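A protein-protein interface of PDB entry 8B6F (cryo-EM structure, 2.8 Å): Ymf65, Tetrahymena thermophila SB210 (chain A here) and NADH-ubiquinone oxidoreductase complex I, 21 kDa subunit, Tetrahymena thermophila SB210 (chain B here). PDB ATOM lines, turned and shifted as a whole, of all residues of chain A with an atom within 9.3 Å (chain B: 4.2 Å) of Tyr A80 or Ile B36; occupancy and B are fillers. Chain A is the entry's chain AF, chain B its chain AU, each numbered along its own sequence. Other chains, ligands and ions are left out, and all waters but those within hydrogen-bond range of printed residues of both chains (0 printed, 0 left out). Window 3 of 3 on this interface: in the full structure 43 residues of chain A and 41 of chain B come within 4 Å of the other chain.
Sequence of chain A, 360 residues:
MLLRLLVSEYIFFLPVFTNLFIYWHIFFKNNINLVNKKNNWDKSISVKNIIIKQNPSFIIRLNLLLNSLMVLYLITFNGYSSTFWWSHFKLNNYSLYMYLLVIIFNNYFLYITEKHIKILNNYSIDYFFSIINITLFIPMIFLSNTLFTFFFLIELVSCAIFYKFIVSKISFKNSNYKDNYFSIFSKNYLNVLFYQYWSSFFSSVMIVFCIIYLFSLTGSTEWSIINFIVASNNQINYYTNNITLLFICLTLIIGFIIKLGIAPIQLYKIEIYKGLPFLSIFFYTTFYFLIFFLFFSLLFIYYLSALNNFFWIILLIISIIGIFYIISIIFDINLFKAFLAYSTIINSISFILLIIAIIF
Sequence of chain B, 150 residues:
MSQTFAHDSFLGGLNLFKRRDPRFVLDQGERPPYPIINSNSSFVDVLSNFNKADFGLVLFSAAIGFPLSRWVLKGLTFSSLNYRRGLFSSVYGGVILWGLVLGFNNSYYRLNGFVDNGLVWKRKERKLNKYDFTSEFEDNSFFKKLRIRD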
ATOM      1  N   SER A   8      -1.490 -16.169   0.317  1.00  0.00           N
ATOM      2  CA  SER A   8      -2.857 -16.165   0.819  1.00  0.00           C
ATOM      3  C   SER A   8      -2.895 -16.214   2.340  1.00  0.00           C
ATOM      4  O   SER A   8      -3.859 -15.739   2.949  1.00  0.00           O
ATOM      5  CB  SER A   8      -3.634 -17.341   0.230  1.00  0.00           C
ATOM      6  OG  SER A   8      -2.990 -18.570   0.516  1.00  0.00           O
ATOM      7  N   ILE A  11      -1.809 -12.221   3.196  1.00  0.00           N
ATOM      8  CA  ILE A  11      -2.134 -11.054   2.382  1.00  0.00           C
ATOM      9  C   ILE A  11      -2.842  -9.993   3.219  1.00  0.00           C
ATOM     10  O   ILE A  11      -2.551  -8.797   3.102  1.00  0.00           O
ATOM     11  CB  ILE A  11      -2.971 -11.474   1.156  1.00  0.00           C
ATOM     12  CG1 ILE A  11      -3.163 -10.296   0.196  1.00  0.00           C
ATOM     13  CG2 ILE A  11      -4.326 -12.024   1.575  1.00  0.00           C
ATOM     14  CD1 ILE A  11      -1.883  -9.795  -0.441  1.00  0.00           C
ATOM     15  N   PHE A  77     -11.106  -5.161  -1.898  1.00  0.00           N
ATOM     16  CA  PHE A  77     -10.671  -6.491  -1.499  1.00  0.00           C
ATOM     17  C   PHE A  77     -11.269  -7.563  -2.405  1.00  0.00           C
ATOM     18  O   PHE A  77     -12.392  -7.440  -2.897  1.00  0.00           O
ATOM     19  CB  PHE A  77     -11.063  -6.755  -0.045  1.00  0.00           C
ATOM     20  CG  PHE A  77     -10.458  -7.999   0.527  1.00  0.00           C
ATOM     21  CD1 PHE A  77      -9.211  -7.964   1.124  1.00  0.00           C
ATOM     22  CD2 PHE A  77     -11.135  -9.204   0.468  1.00  0.00           C
ATOM     23  CE1 PHE A  77      -8.650  -9.105   1.651  1.00  0.00           C
ATOM     24  CE2 PHE A  77     -10.577 -10.350   0.994  1.00  0.00           C
ATOM     25  CZ  PHE A  77      -9.333 -10.299   1.586  1.00  0.00           C
ATOM     26  N   ASN A  78     -10.492  -8.623  -2.621  1.00  0.00           N
ATOM     27  CA  ASN A  78     -10.933  -9.789  -3.373  1.00  0.00           C
ATOM     28  C   ASN A  78     -10.293 -11.027  -2.761  1.00  0.00           C
ATOM     29  O   ASN A  78      -9.278 -10.944  -2.068  1.00  0.00           O
ATOM     30  CB  ASN A  78     -10.560  -9.689  -4.857  1.00  0.00           C
ATOM     31  CG  ASN A  78     -11.278  -8.564  -5.566  1.00  0.00           C
ATOM     32  OD1 ASN A  78     -12.460  -8.322  -5.335  1.00  0.00           O
ATOM     33  ND2 ASN A  78     -10.564  -7.867  -6.439  1.00  0.00           N
ATOM     34  N   GLY A  79     -10.896 -12.172  -3.020  1.00  0.00           N
ATOM     35  CA  GLY A  79     -10.343 -13.430  -2.560  1.00  0.00           C
ATOM     36  C   GLY A  79     -11.425 -14.478  -2.414  1.00  0.00           C
ATOM     37  O   GLY A  79     -12.601 -14.234  -2.661  1.00  0.00           O
ATOM     38  N   TYR A  80     -10.989 -15.668  -2.011  1.00  0.00           N
ATOM     39  CA  TYR A  80     -11.896 -16.759  -1.687  1.00  0.00           C
ATOM     40  C   TYR A  80     -12.311 -16.670  -0.225  1.00  0.00           C
ATOM     41  O   TYR A  80     -11.585 -16.134   0.615  1.00  0.00           O
ATOM     42  CB  TYR A  80     -11.242 -18.117  -1.945  1.00  0.00           C
ATOM     43  CG  TYR A  80     -10.791 -18.342  -3.369  1.00  0.00           C
ATOM     44  CD1 TYR A  80     -11.692 -18.716  -4.356  1.00  0.00           C
ATOM     45  CD2 TYR A  80      -9.456 -18.208  -3.719  1.00  0.00           C
ATOM     46  CE1 TYR A  80     -11.279 -18.932  -5.654  1.00  0.00           C
ATOM     47  CE2 TYR A  80      -9.031 -18.423  -5.011  1.00  0.00           C
ATOM     48  CZ  TYR A  80      -9.946 -18.785  -5.975  1.00  0.00           C
ATOM     49  OH  TYR A  80      -9.519 -18.997  -7.263  1.00  0.00           O
ATOM     50  N   SER A  81     -13.488 -17.209   0.074  1.00  0.00           N
ATOM     51  CA  SER A  81     -13.973 -17.266   1.447  1.00  0.00           C
ATOM     52  C   SER A  81     -13.370 -18.493   2.119  1.00  0.00           C
ATOM     53  O   SER A  81     -13.734 -19.627   1.795  1.00  0.00           O
ATOM     54  CB  SER A  81     -15.498 -17.305   1.484  1.00  0.00           C
ATOM     55  OG  SER A  81     -15.994 -18.485   0.878  1.00  0.00           O
ATOM     56  N   SER A  82     -12.444 -18.272   3.043  1.00  0.00           N
ATOM     57  CA  SER A  82     -11.757 -19.361   3.731  1.00  0.00           C
ATOM     58  C   SER A  82     -10.989 -18.766   4.904  1.00  0.00           C
ATOM     59  O   SER A  82     -11.070 -17.566   5.183  1.00  0.00           O
ATOM     60  CB  SER A  82     -10.823 -20.119   2.784  1.00  0.00           C
ATOM     61  OG  SER A  82     -11.542 -20.704   1.712  1.00  0.00           O
ATOM     62  N   THR A  83     -10.242 -19.621   5.593  1.00  0.00           N
ATOM     63  CA  THR A  83      -9.410 -19.217   6.716  1.00  0.00           C
ATOM     64  C   THR A  83      -7.963 -19.087   6.266  1.00  0.00           C
ATOM     65  O   THR A  83      -7.530 -19.745   5.318  1.00  0.00           O
ATOM     66  CB  THR A  83      -9.504 -20.228   7.861  1.00  0.00           C
ATOM     67  OG1 THR A  83      -8.937 -21.479   7.452  1.00  0.00           O
ATOM     68  CG2 THR A  83     -10.948 -20.442   8.273  1.00  0.00           C
ATOM     69  N   PHE A  84      -7.214 -18.230   6.958  1.00  0.00           N
ATOM     70  CA  PHE A  84      -5.821 -17.993   6.614  1.00  0.00           C
ATOM     71  C   PHE A  84      -4.971 -17.979   7.878  1.00  0.00           C
ATOM     72  O   PHE A  84      -5.455 -17.719   8.981  1.00  0.00           O
ATOM     73  CB  PHE A  84      -5.644 -16.681   5.832  1.00  0.00           C
ATOM     74  CG  PHE A  84      -6.042 -15.450   6.595  1.00  0.00           C
ATOM     75  CD1 PHE A  84      -7.370 -15.069   6.678  1.00  0.00           C
ATOM     76  CD2 PHE A  84      -5.084 -14.661   7.209  1.00  0.00           C
ATOM     77  CE1 PHE A  84      -7.736 -13.933   7.372  1.00  0.00           C
ATOM     78  CE2 PHE A  84      -5.444 -13.524   7.903  1.00  0.00           C
ATOM     79  CZ  PHE A  84      -6.771 -13.158   7.985  1.00  0.00           C
ATOM     80  N   PHE A  89      -7.681 -17.251  11.530  1.00  0.00           N
ATOM     81  CA  PHE A  89      -8.486 -16.118  11.099  1.00  0.00           C
ATOM     82  C   PHE A  89      -9.422 -16.559   9.987  1.00  0.00           C
ATOM     83  O   PHE A  89      -9.029 -17.321   9.100  1.00  0.00           O
ATOM     84  CB  PHE A  89      -7.606 -14.964  10.615  1.00  0.00           C
ATOM     85  CG  PHE A  89      -6.771 -14.348  11.696  1.00  0.00           C
ATOM     86  CD1 PHE A  89      -5.511 -14.844  11.983  1.00  0.00           C
ATOM     87  CD2 PHE A  89      -7.247 -13.273  12.426  1.00  0.00           C
ATOM     88  CE1 PHE A  89      -4.741 -14.278  12.977  1.00  0.00           C
ATOM     89  CE2 PHE A  89      -6.483 -12.704  13.421  1.00  0.00           C
ATOM     90  CZ  PHE A  89      -5.228 -13.206  13.698  1.00  0.00           C
ATOM     91  N   LYS A  90     -10.662 -16.083  10.042  1.00  0.00           N
ATOM     92  CA  LYS A  90     -11.666 -16.391   9.037  1.00  0.00           C
ATOM     93  C   LYS A  90     -11.832 -15.207   8.096  1.00  0.00           C
ATOM     94  O   LYS A  90     -11.833 -14.052   8.529  1.00  0.00           O
ATOM     95  CB  LYS A  90     -13.007 -16.736   9.688  1.00  0.00           C
ATOM     96  CG  LYS A  90     -14.158 -16.949   8.704  1.00  0.00           C
ATOM     97  CD  LYS A  90     -13.902 -18.101   7.739  1.00  0.00           C
ATOM     98  CE  LYS A  90     -14.040 -19.454   8.416  1.00  0.00           C
ATOM     99  NZ  LYS A  90     -15.440 -19.728   8.840  1.00  0.00           N
ATOM    100  N   LEU A  91     -11.969 -15.502   6.806  1.00  0.00           N
ATOM    101  CA  LEU A  91     -12.085 -14.489   5.758  1.00  0.00           C
ATOM    102  C   LEU A  91     -13.345 -14.802   4.957  1.00  0.00           C
ATOM    103  O   LEU A  91     -13.299 -15.581   4.005  1.00  0.00           O
ATOM    104  CB  LEU A  91     -10.841 -14.489   4.880  1.00  0.00           C
ATOM    105  CG  LEU A  91     -10.696 -13.336   3.892  1.00  0.00           C
ATOM    106  CD1 LEU A  91     -10.317 -12.063   4.632  1.00  0.00           C
ATOM    107  CD2 LEU A  91      -9.667 -13.682   2.830  1.00  0.00           C
ATOM    108  N   ASN A  92     -14.468 -14.202   5.344  1.00  0.00           N
ATOM    109  CA  ASN A  92     -15.727 -14.407   4.646  1.00  0.00           C
ATOM    110  C   ASN A  92     -16.497 -13.095   4.610  1.00  0.00           C
ATOM    111  O   ASN A  92     -16.114 -12.104   5.236  1.00  0.00           O
ATOM    112  CB  ASN A  92     -16.565 -15.517   5.295  1.00  0.00           C
ATOM    113  CG  ASN A  92     -16.860 -15.253   6.754  1.00  0.00           C
ATOM    114  OD1 ASN A  92     -16.672 -14.145   7.247  1.00  0.00           O
ATOM    115  ND2 ASN A  92     -17.333 -16.275   7.454  1.00  0.00           N
ATOM    116  N   ASN A  93     -17.601 -13.100   3.859  1.00  0.00           N
ATOM    117  CA  ASN A  93     -18.321 -11.861   3.586  1.00  0.00           C
ATOM    118  C   ASN A  93     -18.842 -11.219   4.866  1.00  0.00           C
ATOM    119  O   ASN A  93     -18.717 -10.004   5.052  1.00  0.00           O
ATOM    120  CB  ASN A  93     -19.470 -12.130   2.616  1.00  0.00           C
ATOM    121  CG  ASN A  93     -18.984 -12.558   1.248  1.00  0.00           C
ATOM    122  OD1 ASN A  93     -17.971 -12.069   0.757  1.00  0.00           O
ATOM    123  ND2 ASN A  93     -19.704 -13.480   0.627  1.00  0.00           N
ATOM    124  N   LEU A  96     -15.950  -9.771   7.025  1.00  0.00           N
ATOM    125  CA  LEU A  96     -15.408  -8.569   6.402  1.00  0.00           C
ATOM    126  C   LEU A  96     -16.371  -7.397   6.526  1.00  0.00           C
ATOM    127  O   LEU A  96     -15.945  -6.258   6.749  1.00  0.00           O
ATOM    128  CB  LEU A  96     -15.068  -8.844   4.937  1.00  0.00           C
ATOM    129  CG  LEU A  96     -13.892  -9.800   4.722  1.00  0.00           C
ATOM    130  CD1 LEU A  96     -13.744 -10.156   3.260  1.00  0.00           C
ATOM    131  CD2 LEU A  96     -12.599  -9.192   5.245  1.00  0.00           C
ATOM    132  N   VAL B  25     -15.733 -11.605  -1.001  1.00  0.00           N
ATOM    133  CA  VAL B  25     -14.975 -12.759  -1.458  1.00  0.00           C
ATOM    134  C   VAL B  25     -15.921 -13.749  -2.124  1.00  0.00           C
ATOM    135  O   VAL B  25     -17.127 -13.762  -1.873  1.00  0.00           O
ATOM    136  CB  VAL B  25     -14.217 -13.441  -0.300  1.00  0.00           C
ATOM    137  CG1 VAL B  25     -13.085 -12.558   0.185  1.00  0.00           C
ATOM    138  CG2 VAL B  25     -15.167 -13.754   0.842  1.00  0.00           C
ATOM    139  N   LEU B  26     -15.351 -14.581  -2.989  1.00  0.00           N
ATOM    140  CA  LEU B  26     -16.106 -15.642  -3.631  1.00  0.00           C
ATOM    141  C   LEU B  26     -16.278 -16.821  -2.678  1.00  0.00           C
ATOM    142  O   LEU B  26     -15.553 -16.969  -1.691  1.00  0.00           O
ATOM    143  CB  LEU B  26     -15.405 -16.107  -4.909  1.00  0.00           C
ATOM    144  CG  LEU B  26     -15.135 -15.032  -5.962  1.00  0.00           C
ATOM    145  CD1 LEU B  26     -14.350 -15.613  -7.120  1.00  0.00           C
ATOM    146  CD2 LEU B  26     -16.431 -14.415  -6.458  1.00  0.00           C
ATOM    147  N   ASP B  27     -17.254 -17.666  -2.986  1.00  0.00           N
ATOM    148  CA  ASP B  27     -17.470 -18.865  -2.195  1.00  0.00           C
ATOM    149  C   ASP B  27     -16.340 -19.863  -2.426  1.00  0.00           C
ATOM    150  O   ASP B  27     -15.588 -19.780  -3.398  1.00  0.00           O
ATOM    151  CB  ASP B  27     -18.812 -19.509  -2.544  1.00  0.00           C
ATOM    152  CG  ASP B  27     -19.992 -18.620  -2.210  1.00  0.00           C
ATOM    153  OD1 ASP B  27     -20.231 -17.642  -2.948  1.00  0.00           O
ATOM    154  OD2 ASP B  27     -20.682 -18.898  -1.207  1.00  0.00           O
ATOM    155  N   GLU B  30     -16.365 -21.479  -6.027  1.00  0.00           N
ATOM    156  CA  GLU B  30     -16.831 -20.657  -7.133  1.00  0.00           C
ATOM    157  C   GLU B  30     -15.658 -20.280  -8.029  1.00  0.00           C
ATOM    158  O   GLU B  30     -14.604 -19.863  -7.543  1.00  0.00           O
ATOM    159  CB  GLU B  30     -17.526 -19.402  -6.608  1.00  0.00           C
ATOM    160  CG  GLU B  30     -18.136 -18.538  -7.695  1.00  0.00           C
ATOM    161  CD  GLU B  30     -18.906 -17.363  -7.133  1.00  0.00           C
ATOM    162  OE1 GLU B  30     -19.018 -17.264  -5.893  1.00  0.00           O
ATOM    163  OE2 GLU B  30     -19.399 -16.536  -7.927  1.00  0.00           O
ATOM    164  N   PRO B  32     -13.202 -18.273 -10.367  1.00  0.00           N
ATOM    165  CA  PRO B  32     -12.897 -16.856 -10.526  1.00  0.00           C
ATOM    166  C   PRO B  32     -13.365 -16.354 -11.876  1.00  0.00           C
ATOM    167  O   PRO B  32     -13.484 -17.133 -12.841  1.00  0.00           O
ATOM    168  CB  PRO B  32     -11.368 -16.806 -10.404  1.00  0.00           C
ATOM    169  CG  PRO B  32     -11.006 -18.016  -9.659  1.00  0.00           C
ATOM    170  CD  PRO B  32     -11.991 -19.058 -10.074  1.00  0.00           C
ATOM    171  N   TYR B  34     -11.883 -14.783 -14.173  1.00  0.00           N
ATOM    172  CA  TYR B  34     -10.866 -14.861 -15.207  1.00  0.00           C
ATOM    173  C   TYR B  34      -9.984 -16.084 -14.993  1.00  0.00           C
ATOM    174  O   TYR B  34      -9.884 -16.599 -13.874  1.00  0.00           O
ATOM    175  CB  TYR B  34      -9.997 -13.594 -15.213  1.00  0.00           C
ATOM    176  CG  TYR B  34     -10.786 -12.323 -15.420  1.00  0.00           C
ATOM    177  CD1 TYR B  34     -11.131 -11.896 -16.694  1.00  0.00           C
ATOM    178  CD2 TYR B  34     -11.186 -11.551 -14.338  1.00  0.00           C
ATOM    179  CE1 TYR B  34     -11.853 -10.736 -16.884  1.00  0.00           C
ATOM    180  CE2 TYR B  34     -11.909 -10.390 -14.520  1.00  0.00           C
ATOM    181  CZ  TYR B  34     -12.239  -9.987 -15.794  1.00  0.00           C
ATOM    182  OH  TYR B  34     -12.958  -8.832 -15.977  1.00  0.00           O
ATOM    183  N   PRO B  35      -9.332 -16.579 -16.045  1.00  0.00           N
ATOM    184  CA  PRO B  35      -8.482 -17.765 -15.889  1.00  0.00           C
ATOM    185  C   PRO B  35      -7.403 -17.554 -14.837  1.00  0.00           C
ATOM    186  O   PRO B  35      -6.829 -16.471 -14.714  1.00  0.00           O
ATOM    187  CB  PRO B  35      -7.881 -17.955 -17.286  1.00  0.00           C
ATOM    188  CG  PRO B  35      -8.862 -17.328 -18.199  1.00  0.00           C
ATOM    189  CD  PRO B  35      -9.430 -16.159 -17.453  1.00  0.00           C
ATOM    190  N   ILE B  36      -7.137 -18.607 -14.073  1.00  0.00           N
ATOM    191  CA  ILE B  36      -6.145 -18.553 -13.005  1.00  0.00           C
ATOM    192  C   ILE B  36      -4.756 -18.696 -13.611  1.00  0.00           C
ATOM    193  O   ILE B  36      -4.492 -19.626 -14.381  1.00  0.00           O
ATOM    194  CB  ILE B  36      -6.411 -19.652 -11.964  1.00  0.00           C
ATOM    195  CG1 ILE B  36      -7.777 -19.434 -11.308  1.00  0.00           C
ATOM    196  CG2 ILE B  36      -5.309 -19.675 -10.909  1.00  0.00           C
ATOM    197  CD1 ILE B  36      -8.214 -20.568 -10.404  1.00  0.00           C
ATOM    198  N   ILE B  37      -3.864 -17.773 -13.263  1.00  0.00           N
ATOM    199  CA  ILE B  37      -2.483 -17.837 -13.729  1.00  0.00           C
ATOM    200  C   ILE B  37      -1.602 -18.583 -12.738  1.00  0.00           C
ATOM    201  O   ILE B  37      -0.767 -19.398 -13.134  1.00  0.00           O
ATOM    202  CB  ILE B  37      -1.957 -16.411 -13.989  1.00  0.00           C
ATOM    203  CG1 ILE B  37      -2.757 -15.749 -15.111  1.00  0.00           C
ATOM    204  CG2 ILE B  37      -0.474 -16.439 -14.337  1.00  0.00           C
ATOM    205  CD1 ILE B  37      -2.500 -14.265 -15.254  1.00  0.00           C
ATOM    206  N   ASN B  38      -1.770 -18.319 -11.443  1.00  0.00           N
ATOM    207  CA  ASN B  38      -1.001 -19.015 -10.416  1.00  0.00           C
ATOM    208  C   ASN B  38      -1.808 -18.971  -9.128  1.00  0.00           C
ATOM    209  O   ASN B  38      -1.919 -17.910  -8.505  1.00  0.00           O
ATOM    210  CB  ASN B  38       0.367 -18.371 -10.232  1.00  0.00           C
ATOM    211  CG  ASN B  38       1.212 -19.083  -9.196  1.00  0.00           C
ATOM    212  OD1 ASN B  38       0.927 -20.216  -8.816  1.00  0.00           O
ATOM    213  ND2 ASN B  38       2.262 -18.417  -8.734  1.00  0.00           N
ATOM    214  N   SER B  39      -2.373 -20.112  -8.736  1.00  0.00           N
ATOM    215  CA  SER B  39      -3.174 -20.154  -7.518  1.00  0.00           C
ATOM    216  C   SER B  39      -2.303 -20.059  -6.273  1.00  0.00           C
ATOM    217  O   SER B  39      -2.622 -19.313  -5.340  1.00  0.00           O
ATOM    218  CB  SER B  39      -4.008 -21.430  -7.477  1.00  0.00           C
ATOM    219  OG  SER B  39      -4.682 -21.514  -6.235  1.00  0.00           O
ATOM    220  N   LEU B 111      -2.900 -12.437 -10.682  1.00  0.00           N
ATOM    221  CA  LEU B 111      -2.413 -13.812 -10.693  1.00  0.00           C
ATOM    222  C   LEU B 111      -3.542 -14.797 -10.416  1.00  0.00           C
ATOM    223  O   LEU B 111      -3.635 -15.844 -11.066  1.00  0.00           O
ATOM    224  CB  LEU B 111      -1.295 -13.977  -9.662  1.00  0.00           C
ATOM    225  CG  LEU B 111       0.091 -13.467 -10.064  1.00  0.00           C
ATOM    226  CD1 LEU B 111       1.029 -13.489  -8.876  1.00  0.00           C
ATOM    227  CD2 LEU B 111       0.667 -14.287 -11.203  1.00  0.00           C
ATOM    228  N   ASN B 112      -4.408 -14.484  -9.453  1.00  0.00           N
ATOM    229  CA  ASN B 112      -5.470 -15.401  -9.063  1.00  0.00           C
ATOM    230  C   ASN B 112      -6.700 -15.322  -9.957  1.00  0.00           C
ATOM    231  O   ASN B 112      -7.612 -16.137  -9.792  1.00  0.00           O
ATOM    232  CB  ASN B 112      -5.882 -15.132  -7.615  1.00  0.00           C
ATOM    233  CG  ASN B 112      -4.875 -15.658  -6.618  1.00  0.00           C
ATOM    234  OD1 ASN B 112      -5.024 -16.756  -6.088  1.00  0.00           O
ATOM    235  ND2 ASN B 112      -3.835 -14.875  -6.362  1.00  0.00           N
ATOM    236  N   PHE B 114      -8.899 -12.853 -10.011  1.00  0.00           N
ATOM    237  CA  PHE B 114      -9.991 -12.081  -9.425  1.00  0.00           C
ATOM    238  C   PHE B 114     -10.312 -10.851 -10.263  1.00  0.00           C
ATOM    239  O   PHE B 114     -11.485 -10.516 -10.460  1.00  0.00           O
ATOM    240  CB  PHE B 114      -9.636 -11.677  -7.994  1.00  0.00           C
ATOM    241  CG  PHE B 114      -9.330 -12.841  -7.096  1.00  0.00           C
ATOM    242  CD1 PHE B 114     -10.054 -14.017  -7.191  1.00  0.00           C
ATOM    243  CD2 PHE B 114      -8.313 -12.761  -6.164  1.00  0.00           C
ATOM    244  CE1 PHE B 114      -9.772 -15.086  -6.369  1.00  0.00           C
ATOM    245  CE2 PHE B 114      -8.026 -13.825  -5.339  1.00  0.00           C
ATOM    246  CZ  PHE B 114      -8.756 -14.990  -5.441  1.00  0.00           C
ATOM    247  N   TRP B 121     -12.012 -17.252 -19.793  1.00  0.00           N
ATOM    248  CA  TRP B 121     -12.341 -18.670 -19.794  1.00  0.00           C
ATOM    249  C   TRP B 121     -12.897 -19.081 -21.152  1.00  0.00           C
ATOM    250  O   TRP B 121     -13.599 -18.317 -21.818  1.00  0.00           O
ATOM    251  CB  TRP B 121     -13.361 -18.989 -18.701  1.00  0.00           C
ATOM    252  CG  TRP B 121     -12.870 -18.754 -17.308  1.00  0.00           C
ATOM    253  CD1 TRP B 121     -13.147 -17.682 -16.514  1.00  0.00           C
ATOM    254  CD2 TRP B 121     -12.022 -19.617 -16.540  1.00  0.00           C
ATOM    255  NE1 TRP B 121     -12.522 -17.821 -15.298  1.00  0.00           N
ATOM    256  CE2 TRP B 121     -11.824 -19.001 -15.289  1.00  0.00           C
ATOM    257  CE3 TRP B 121     -11.411 -20.849 -16.790  1.00  0.00           C
ATOM    258  CZ2 TRP B 121     -11.043 -19.575 -14.289  1.00  0.00           C
ATOM    259  CZ3 TRP B 121     -10.634 -21.419 -15.796  1.00  0.00           C
ATOM    260  CH2 TRP B 121     -10.457 -20.781 -14.560  1.00  0.00           C
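Of the 15 printed residues of chain B, 7 touch a printed residue of chain A. Printed residues of chain B that touch a printed residue of chain A: Val B25, Leu B26, Asp B27, Glu B30, Pro B32, Ile B36 and Phe B114. Hydrophobic or aromatic side chains of chain B within 4 Å of the printed part of chain A: Val B25, Pro B32, Ile B36 and Phe B114. Among the printed residues, 17 pairs touch across the chains. Among the printed residues, no Asp or Glu carboxylate lies within 4 Å of a Lys or Arg side-chain nitrogen of the other chain.
Of the printed residues of chain B, Gly A79 touches Val B25, Leu B26 and Phe B114. Of the printed residues of chain B, Tyr A80 touches Val B25, Leu B26, Glu B30, Pro B32, Ile B36 and Phe B114. Lys A90 touches none of the printed residues of chain B. Of the printed residues of chain A, Pro B32 touches Tyr A80. No residue of chain A comes within 4 Å of Pro B35. Ile B36 touches one residue of chain A. No residue of chain A comes within 4 Å of Ile B37. Ser B39 touches none of the printed residues of chain A. The nearest printed residue of chain A that does not touch Ile B36 is Gly A79 (10.5 Å). The nearest printed residue of chain A that does not touch Asp B27 is Tyr A80 (4.2 Å).
O of Pro B32 is in hydrogen-bond range of NE1 of Trp B121 (2.7 Å). The backbone NH of Asp B27 is in hydrogen-bond range of the side-chain carboxylate of Glu B30 (3.4 Å).
Phe A77 touches Val B25 (CE2 to CG1, 3.4 Å). CB of Asn A78 touches CB of Phe B114, at 3.8 Å. Gly A79 touches Val B25 (O to CB, 3.0 Å). CA of Gly A79 touches CE2 of Phe B114, 3.6 Å away. Tyr A80 touches Val B25 (C to CB, 3.8 Å). Tyr A80 touches Leu B26 (C to O, 3.6 Å). Tyr A80 touches Glu B30. Tyr A80 touches Pro B32 (OH to CG, 3.0 Å). CD1 of Ile B36 touches OH of Tyr A80 (3.7 Å). CG2 of Val B25 touches CA of Asn A92, at 3.9 Å.
The side-chain amide oxygen (OD1) of Asn A93 is in hydrogen-bond range of the backbone NH (N) of Val B25 (2.9 Å). The backbone NH (N) of Ser A81 lies within hydrogen-bond range of the backbone carbonyl oxygen (O) of Leu B26, at 2.7 Å. The backbone carbonyl oxygen of Gly A79 sits at hydrogen-bond distance from the backbone NH of Leu B26 (2.8 Å).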
